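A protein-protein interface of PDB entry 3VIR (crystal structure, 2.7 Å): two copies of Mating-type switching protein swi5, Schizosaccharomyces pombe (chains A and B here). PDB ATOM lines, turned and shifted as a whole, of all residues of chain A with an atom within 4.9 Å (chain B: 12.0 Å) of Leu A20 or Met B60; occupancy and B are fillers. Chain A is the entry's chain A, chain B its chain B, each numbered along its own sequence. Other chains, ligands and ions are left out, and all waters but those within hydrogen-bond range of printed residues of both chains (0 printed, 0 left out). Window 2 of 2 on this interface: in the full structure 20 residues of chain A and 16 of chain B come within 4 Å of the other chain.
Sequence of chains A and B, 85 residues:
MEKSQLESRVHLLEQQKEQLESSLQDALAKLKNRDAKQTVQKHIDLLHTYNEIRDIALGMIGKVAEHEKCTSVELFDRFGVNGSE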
ATOM      1  N   GLN A  16     -13.390 -28.718  21.120  1.00  0.00           N
ATOM      2  CA  GLN A  16     -14.039 -27.430  21.354  1.00  0.00           C
ATOM      3  C   GLN A  16     -14.092 -26.573  20.098  1.00  0.00           C
ATOM      4  O   GLN A  16     -14.913 -25.637  19.997  1.00  0.00           O
ATOM      5  CB  GLN A  16     -13.300 -26.663  22.452  1.00  0.00           C
ATOM      6  CG  GLN A  16     -13.550 -27.166  23.869  1.00  0.00           C
ATOM      7  CD  GLN A  16     -12.560 -26.596  24.872  1.00  0.00           C
ATOM      8  OE1 GLN A  16     -11.780 -25.687  24.560  1.00  0.00           O
ATOM      9  NE2 GLN A  16     -12.583 -27.133  26.083  1.00  0.00           N
ATOM     10  N   LYS A  17     -13.198 -26.869  19.158  1.00  0.00           N
ATOM     11  CA  LYS A  17     -13.232 -26.231  17.847  1.00  0.00           C
ATOM     12  C   LYS A  17     -14.434 -26.767  17.040  1.00  0.00           C
ATOM     13  O   LYS A  17     -15.197 -25.979  16.503  1.00  0.00           O
ATOM     14  CB  LYS A  17     -11.892 -26.409  17.128  1.00  0.00           C
ATOM     15  CG  LYS A  17     -11.660 -25.527  15.911  1.00  0.00           C
ATOM     16  CD  LYS A  17     -10.144 -25.306  15.560  1.00  0.00           C
ATOM     17  CE  LYS A  17      -9.351 -26.588  15.091  1.00  0.00           C
ATOM     18  NZ  LYS A  17      -7.860 -26.554  15.404  1.00  0.00           N
ATOM     19  N   GLU A  18     -14.652 -28.083  16.995  1.00  0.00           N
ATOM     20  CA  GLU A  18     -15.783 -28.622  16.210  1.00  0.00           C
ATOM     21  C   GLU A  18     -17.192 -28.391  16.793  1.00  0.00           C
ATOM     22  O   GLU A  18     -18.141 -28.325  16.034  1.00  0.00           O
ATOM     23  CB  GLU A  18     -15.593 -30.105  15.883  1.00  0.00           C
ATOM     24  CG  GLU A  18     -14.767 -30.364  14.622  1.00  0.00           C
ATOM     25  CD  GLU A  18     -13.408 -31.031  14.898  1.00  0.00           C
ATOM     26  OE1 GLU A  18     -12.409 -30.702  14.203  1.00  0.00           O
ATOM     27  OE2 GLU A  18     -13.345 -31.903  15.797  1.00  0.00           O
ATOM     28  N   GLN A  19     -17.342 -28.281  18.113  1.00  0.00           N
ATOM     29  CA  GLN A  19     -18.662 -28.001  18.694  1.00  0.00           C
ATOM     30  C   GLN A  19     -19.024 -26.554  18.405  1.00  0.00           C
ATOM     31  O   GLN A  19     -20.192 -26.214  18.194  1.00  0.00           O
ATOM     32  CB  GLN A  19     -18.709 -28.241  20.204  1.00  0.00           C
ATOM     33  CG  GLN A  19     -20.148 -28.419  20.748  1.00  0.00           C
ATOM     34  CD  GLN A  19     -20.206 -28.545  22.286  1.00  0.00           C
ATOM     35  OE1 GLN A  19     -19.451 -29.317  22.891  1.00  0.00           O
ATOM     36  NE2 GLN A  19     -21.113 -27.783  22.918  1.00  0.00           N
ATOM     37  N   LEU A  20     -18.005 -25.707  18.412  1.00  0.00           N
ATOM     38  CA  LEU A  20     -18.149 -24.322  18.017  1.00  0.00           C
ATOM     39  C   LEU A  20     -18.589 -24.267  16.567  1.00  0.00           C
ATOM     40  O   LEU A  20     -19.600 -23.634  16.246  1.00  0.00           O
ATOM     41  CB  LEU A  20     -16.806 -23.610  18.198  1.00  0.00           C
ATOM     42  CG  LEU A  20     -16.669 -22.158  17.798  1.00  0.00           C
ATOM     43  CD1 LEU A  20     -17.510 -21.325  18.740  1.00  0.00           C
ATOM     44  CD2 LEU A  20     -15.200 -21.743  17.816  1.00  0.00           C
ATOM     45  N   GLU A  21     -17.844 -24.938  15.687  1.00  0.00           N
ATOM     46  CA  GLU A  21     -18.075 -24.801  14.238  1.00  0.00           C
ATOM     47  C   GLU A  21     -19.452 -25.306  13.860  1.00  0.00           C
ATOM     48  O   GLU A  21     -20.153 -24.692  13.050  1.00  0.00           O
ATOM     49  CB  GLU A  21     -17.009 -25.509  13.399  1.00  0.00           C
ATOM     50  CG  GLU A  21     -17.364 -25.571  11.895  1.00  0.00           C
ATOM     51  CD  GLU A  21     -16.141 -25.697  10.976  1.00  0.00           C
ATOM     52  OE1 GLU A  21     -16.221 -25.197   9.820  1.00  0.00           O
ATOM     53  OE2 GLU A  21     -15.113 -26.286  11.413  1.00  0.00           O
ATOM     54  N   SER A  22     -19.845 -26.422  14.457  1.00  0.00           N
ATOM     55  CA  SER A  22     -21.205 -26.898  14.282  1.00  0.00           C
ATOM     56  C   SER A  22     -22.203 -25.797  14.690  1.00  0.00           C
ATOM     57  O   SER A  22     -22.982 -25.340  13.880  1.00  0.00           O
ATOM     58  CB  SER A  22     -21.431 -28.161  15.096  1.00  0.00           C
ATOM     59  OG  SER A  22     -22.725 -28.651  14.840  1.00  0.00           O
ATOM     60  N   SER A  23     -22.122 -25.366  15.942  1.00  0.00           N
ATOM     61  CA  SER A  23     -22.936 -24.299  16.482  1.00  0.00           C
ATOM     62  C   SER A  23     -22.991 -23.022  15.633  1.00  0.00           C
ATOM     63  O   SER A  23     -24.060 -22.396  15.534  1.00  0.00           O
ATOM     64  CB  SER A  23     -22.437 -23.935  17.879  1.00  0.00           C
ATOM     65  OG  SER A  23     -22.427 -25.064  18.744  1.00  0.00           O
ATOM     66  N   LEU A  24     -21.867 -22.612  15.051  1.00  0.00           N
ATOM     67  CA  LEU A  24     -21.892 -21.484  14.131  1.00  0.00           C
ATOM     68  C   LEU A  24     -22.683 -21.852  12.881  1.00  0.00           C
ATOM     69  O   LEU A  24     -23.704 -21.242  12.617  1.00  0.00           O
ATOM     70  CB  LEU A  24     -20.486 -21.029  13.766  1.00  0.00           C
ATOM     71  CG  LEU A  24     -19.699 -20.468  14.951  1.00  0.00           C
ATOM     72  CD1 LEU A  24     -18.310 -19.862  14.601  1.00  0.00           C
ATOM     73  CD2 LEU A  24     -20.607 -19.431  15.616  1.00  0.00           C
ATOM     74  N   TYR B  50     -30.267 -13.058  17.860  1.00  0.00           N
ATOM     75  CA  TYR B  50     -29.417 -12.367  18.833  1.00  0.00           C
ATOM     76  C   TYR B  50     -29.144 -13.298  20.004  1.00  0.00           C
ATOM     77  O   TYR B  50     -28.023 -13.360  20.484  1.00  0.00           O
ATOM     78  CB  TYR B  50     -30.057 -11.040  19.299  1.00  0.00           C
ATOM     79  CG  TYR B  50     -29.615 -10.577  20.684  1.00  0.00           C
ATOM     80  CD1 TYR B  50     -28.568  -9.669  20.844  1.00  0.00           C
ATOM     81  CD2 TYR B  50     -30.232 -11.074  21.839  1.00  0.00           C
ATOM     82  CE1 TYR B  50     -28.137  -9.268  22.127  1.00  0.00           C
ATOM     83  CE2 TYR B  50     -29.804 -10.691  23.113  1.00  0.00           C
ATOM     84  CZ  TYR B  50     -28.766  -9.774  23.261  1.00  0.00           C
ATOM     85  OH  TYR B  50     -28.368  -9.364  24.534  1.00  0.00           O
ATOM     86  N   ASN B  51     -30.156 -14.021  20.473  1.00  0.00           N
ATOM     87  CA  ASN B  51     -29.914 -15.038  21.509  1.00  0.00           C
ATOM     88  C   ASN B  51     -28.924 -16.178  21.052  1.00  0.00           C
ATOM     89  O   ASN B  51     -27.935 -16.494  21.718  1.00  0.00           O
ATOM     90  CB  ASN B  51     -31.248 -15.593  22.002  1.00  0.00           C
ATOM     91  CG  ASN B  51     -32.007 -14.584  22.853  1.00  0.00           C
ATOM     92  OD1 ASN B  51     -31.454 -13.998  23.790  1.00  0.00           O
ATOM     93  ND2 ASN B  51     -33.277 -14.373  22.531  1.00  0.00           N
ATOM     94  N   GLU B  52     -29.165 -16.766  19.891  1.00  0.00           N
ATOM     95  CA  GLU B  52     -28.267 -17.778  19.402  1.00  0.00           C
ATOM     96  C   GLU B  52     -26.829 -17.250  19.412  1.00  0.00           C
ATOM     97  O   GLU B  52     -25.926 -17.895  19.955  1.00  0.00           O
ATOM     98  CB  GLU B  52     -28.716 -18.250  18.016  1.00  0.00           C
ATOM     99  CG  GLU B  52     -30.016 -19.120  18.082  1.00  0.00           C
ATOM    100  CD  GLU B  52     -30.775 -19.277  16.750  1.00  0.00           C
ATOM    101  OE1 GLU B  52     -30.302 -18.806  15.662  1.00  0.00           O
ATOM    102  OE2 GLU B  52     -31.881 -19.876  16.818  1.00  0.00           O
ATOM    103  N   ILE B  53     -26.602 -16.062  18.879  1.00  0.00           N
ATOM    104  CA  ILE B  53     -25.236 -15.580  18.834  1.00  0.00           C
ATOM    105  C   ILE B  53     -24.769 -15.173  20.207  1.00  0.00           C
ATOM    106  O   ILE B  53     -23.583 -15.232  20.490  1.00  0.00           O
ATOM    107  CB  ILE B  53     -25.053 -14.437  17.889  1.00  0.00           C
ATOM    108  CG1 ILE B  53     -25.468 -14.867  16.475  1.00  0.00           C
ATOM    109  CG2 ILE B  53     -23.600 -13.993  17.890  1.00  0.00           C
ATOM    110  CD1 ILE B  53     -25.833 -13.719  15.575  1.00  0.00           C
ATOM    111  N   ARG B  54     -25.681 -14.780  21.087  1.00  0.00           N
ATOM    112  CA  ARG B  54     -25.277 -14.442  22.465  1.00  0.00           C
ATOM    113  C   ARG B  54     -24.853 -15.707  23.196  1.00  0.00           C
ATOM    114  O   ARG B  54     -23.788 -15.743  23.820  1.00  0.00           O
ATOM    115  CB  ARG B  54     -26.399 -13.728  23.251  1.00  0.00           C
ATOM    116  CG  ARG B  54     -25.941 -13.013  24.557  1.00  0.00           C
ATOM    117  CD  ARG B  54     -27.110 -12.606  25.424  1.00  0.00           C
ATOM    118  NE  ARG B  54     -26.745 -12.550  26.838  1.00  0.00           N
ATOM    119  CZ  ARG B  54     -26.410 -11.446  27.519  1.00  0.00           C
ATOM    120  NH1 ARG B  54     -26.382 -10.241  26.937  1.00  0.00           N
ATOM    121  NH2 ARG B  54     -26.098 -11.552  28.808  1.00  0.00           N
ATOM    122  N   ASP B  55     -25.673 -16.744  23.110  1.00  0.00           N
ATOM    123  CA  ASP B  55     -25.363 -17.990  23.798  1.00  0.00           C
ATOM    124  C   ASP B  55     -24.001 -18.612  23.372  1.00  0.00           C
ATOM    125  O   ASP B  55     -23.227 -19.053  24.237  1.00  0.00           O
ATOM    126  CB  ASP B  55     -26.512 -18.979  23.618  1.00  0.00           C
ATOM    127  CG  ASP B  55     -27.779 -18.532  24.326  1.00  0.00           C
ATOM    128  OD1 ASP B  55     -27.693 -18.249  25.544  1.00  0.00           O
ATOM    129  OD2 ASP B  55     -28.860 -18.471  23.680  1.00  0.00           O
ATOM    130  N   ILE B  56     -23.701 -18.624  22.066  1.00  0.00           N
ATOM    131  CA  ILE B  56     -22.406 -19.127  21.597  1.00  0.00           C
ATOM    132  C   ILE B  56     -21.255 -18.235  22.075  1.00  0.00           C
ATOM    133  O   ILE B  56     -20.166 -18.718  22.326  1.00  0.00           O
ATOM    134  CB  ILE B  56     -22.323 -19.218  20.059  1.00  0.00           C
ATOM    135  CG1 ILE B  56     -23.388 -20.153  19.500  1.00  0.00           C
ATOM    136  CG2 ILE B  56     -20.945 -19.710  19.622  1.00  0.00           C
ATOM    137  CD1 ILE B  56     -23.597 -19.981  18.031  1.00  0.00           C
ATOM    138  N   ALA B  57     -21.492 -16.932  22.175  1.00  0.00           N
ATOM    139  CA  ALA B  57     -20.488 -16.008  22.705  1.00  0.00           C
ATOM    140  C   ALA B  57     -20.164 -16.323  24.170  1.00  0.00           C
ATOM    141  O   ALA B  57     -18.999 -16.438  24.544  1.00  0.00           O
ATOM    142  CB  ALA B  57     -20.966 -14.555  22.565  1.00  0.00           C
ATOM    143  N   LEU B  58     -21.199 -16.455  24.995  1.00  0.00           N
ATOM    144  CA  LEU B  58     -21.017 -16.805  26.404  1.00  0.00           C
ATOM    145  C   LEU B  58     -20.269 -18.122  26.540  1.00  0.00           C
ATOM    146  O   LEU B  58     -19.357 -18.253  27.375  1.00  0.00           O
ATOM    147  CB  LEU B  58     -22.362 -16.930  27.127  1.00  0.00           C
ATOM    148  CG  LEU B  58     -23.121 -15.634  27.373  1.00  0.00           C
ATOM    149  CD1 LEU B  58     -24.365 -15.915  28.257  1.00  0.00           C
ATOM    150  CD2 LEU B  58     -22.198 -14.581  28.000  1.00  0.00           C
ATOM    151  N   GLY B  59     -20.675 -19.099  25.727  1.00  0.00           N
ATOM    152  CA  GLY B  59     -20.056 -20.421  25.751  1.00  0.00           C
ATOM    153  C   GLY B  59     -18.557 -20.262  25.669  1.00  0.00           C
ATOM    154  O   GLY B  59     -17.821 -20.704  26.552  1.00  0.00           O
ATOM    155  N   MET B  60     -18.126 -19.569  24.622  1.00  0.00           N
ATOM    156  CA  MET B  60     -16.719 -19.302  24.397  1.00  0.00           C
ATOM    157  C   MET B  60     -16.084 -18.575  25.575  1.00  0.00           C
ATOM    158  O   MET B  60     -15.057 -19.014  26.093  1.00  0.00           O
ATOM    159  CB  MET B  60     -16.549 -18.521  23.100  1.00  0.00           C
ATOM    160  CG  MET B  60     -16.896 -19.361  21.898  1.00  0.00           C
ATOM    161  SD  MET B  60     -17.145 -18.378  20.435  1.00  0.00           S
ATOM    162  CE  MET B  60     -15.593 -17.530  20.296  1.00  0.00           C
ATOM    163  N   ILE B  61     -16.713 -17.494  26.030  1.00  0.00           N
ATOM    164  CA  ILE B  61     -16.187 -16.763  27.196  1.00  0.00           C
ATOM    165  C   ILE B  61     -16.219 -17.562  28.514  1.00  0.00           C
ATOM    166  O   ILE B  61     -15.373 -17.355  29.379  1.00  0.00           O
ATOM    167  CB  ILE B  61     -16.820 -15.365  27.335  1.00  0.00           C
ATOM    168  CG1 ILE B  61     -15.839 -14.306  26.804  1.00  0.00           C
ATOM    169  CG2 ILE B  61     -17.179 -15.071  28.781  1.00  0.00           C
ATOM    170  CD1 ILE B  61     -14.994 -14.758  25.599  1.00  0.00           C
ATOM    171  N   GLY B  62     -17.163 -18.496  28.640  1.00  0.00           N
ATOM    172  CA  GLY B  62     -17.129 -19.495  29.713  1.00  0.00           C
ATOM    173  C   GLY B  62     -15.986 -20.494  29.576  1.00  0.00           C
ATOM    174  O   GLY B  62     -15.506 -21.013  30.579  1.00  0.00           O
ATOM    175  N   LYS B  63     -15.552 -20.770  28.340  1.00  0.00           N
ATOM    176  CA  LYS B  63     -14.466 -21.740  28.070  1.00  0.00           C
ATOM    177  C   LYS B  63     -13.072 -21.083  28.141  1.00  0.00           C
ATOM    178  O   LYS B  63     -12.161 -21.624  28.790  1.00  0.00           O
ATOM    179  CB  LYS B  63     -14.626 -22.393  26.685  1.00  0.00           C
ATOM    180  CG  LYS B  63     -15.753 -23.421  26.519  1.00  0.00           C
ATOM    181  CD  LYS B  63     -15.734 -24.063  25.083  1.00  0.00           C
ATOM    182  CE  LYS B  63     -15.537 -23.042  23.909  1.00  0.00           C
ATOM    183  NZ  LYS B  63     -15.572 -23.615  22.517  1.00  0.00           N
ATOM    184  N   VAL B  64     -12.906 -19.938  27.462  1.00  0.00           N
ATOM    185  CA  VAL B  64     -11.641 -19.164  27.519  1.00  0.00           C
ATOM    186  C   VAL B  64     -11.340 -18.674  28.956  1.00  0.00           C
ATOM    187  O   VAL B  64     -10.204 -18.322  29.275  1.00  0.00           O
ATOM    188  CB  VAL B  64     -11.632 -17.977  26.506  1.00  0.00           C
ATOM    189  CG1 VAL B  64     -12.791 -17.044  26.781  1.00  0.00           C
ATOM    190  CG2 VAL B  64     -10.313 -17.215  26.544  1.00  0.00           C
ATOM    191  N   ALA B  65     -12.375 -18.647  29.803  1.00  0.00           N
ATOM    192  CA  ALA B  65     -12.220 -18.555  31.261  1.00  0.00           C
ATOM    193  C   ALA B  65     -11.375 -19.718  31.802  1.00  0.00           C
ATOM    194  O   ALA B  65     -10.366 -19.493  32.474  1.00  0.00           O
ATOM    195  CB  ALA B  65     -13.597 -18.545  31.938  1.00  0.00           C
ATOM    196  N   GLU B  66     -11.786 -20.950  31.492  1.00  0.00           N
ATOM    197  CA  GLU B  66     -11.060 -22.172  31.898  1.00  0.00           C
ATOM    198  C   GLU B  66      -9.568 -22.216  31.445  1.00  0.00           C
ATOM    199  O   GLU B  66      -8.658 -22.173  32.284  1.00  0.00           O
ATOM    200  CB  GLU B  66     -11.820 -23.423  31.408  1.00  0.00           C
ATOM    201  N   HIS B  67      -9.330 -22.291  30.134  1.00  0.00           N
ATOM    202  CA  HIS B  67      -7.962 -22.293  29.584  1.00  0.00           C
ATOM    203  C   HIS B  67      -7.252 -20.986  29.934  1.00  0.00           C
ATOM    204  O   HIS B  67      -6.210 -20.667  29.378  1.00  0.00           O
ATOM    205  CB  HIS B  67      -7.967 -22.481  28.056  1.00  0.00           C
ATOM    206  CG  HIS B  67      -8.831 -23.611  27.582  1.00  0.00           C
ATOM    207  ND1 HIS B  67      -8.510 -24.936  27.794  1.00  0.00           N
ATOM    208  CD2 HIS B  67     -10.006 -23.612  26.909  1.00  0.00           C
ATOM    209  CE1 HIS B  67      -9.452 -25.704  27.273  1.00  0.00           C
ATOM    210  NE2 HIS B  67     -10.372 -24.924  26.731  1.00  0.00           N
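Leu A20 touches Ile B56. Leu A20 touches Met B60. CD1 of Ile B56 touches O of Ser A23 (3.5 Å). CD1 of Ile B56 touches CD2 of Leu A24, 3.9 Å away.
Printed residues of chain B within 4 Å of Gln A16: Lys B63 (3.3 Å) and His B67 (2.7 Å). Leu A20 touches two residues of chain B. Ser A22 touches none of the printed residues of chain B. Of chain B, only Ile B56 (3.5 Å) comes within 4 Å of Ser A23. Leu A24 touches one residue of chain B. Printed residues of chain A within 4 Å of Ile B56: Leu A20, Ser A23 and Leu A24. Met B60 touches just one residue of chain A: Leu A20. Printed residues of chain A within 4 Å of Lys B63: Gln A16 (3.3 Å). Printed residues of chain A within 4 Å of His B67: Gln A16. The nearest residue of chain B that does not touch Leu A20 is Lys B63 (4.5 Å).
O of Gln A16 lies within hydrogen-bond range of NZ of Lys B63 (3.3 Å). The side-chain amide oxygen (OE1) of Gln A16 sits at hydrogen-bond distance from a ring nitrogen (NE2) of His B67, at 2.7 Å.
The backbone carbonyl oxygen of Gln A19 sits at hydrogen-bond distance from the side-chain hydroxyl of Ser A23, 2.6 Å away.
Hydrophobic or aromatic side chains of chain A within 4 Å of the printed part of chain B: Leu A20 and Leu A24. Of the 18 printed residues of chain B, 4 touch a printed residue of chain A. Printed residues of chain B that touch a printed residue of chain A: Ile B56, Met B60, Lys B63 and His B67. Hydrophobic or aromatic side chains of chain B within 4 Å of the printed part of chain A: Ile B56, Met B60 and His B67.
No position is printed for both chains. Of the 6 pairs that touch across the chains among the printed residues, none has its exchanged pair printed and touching as well.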
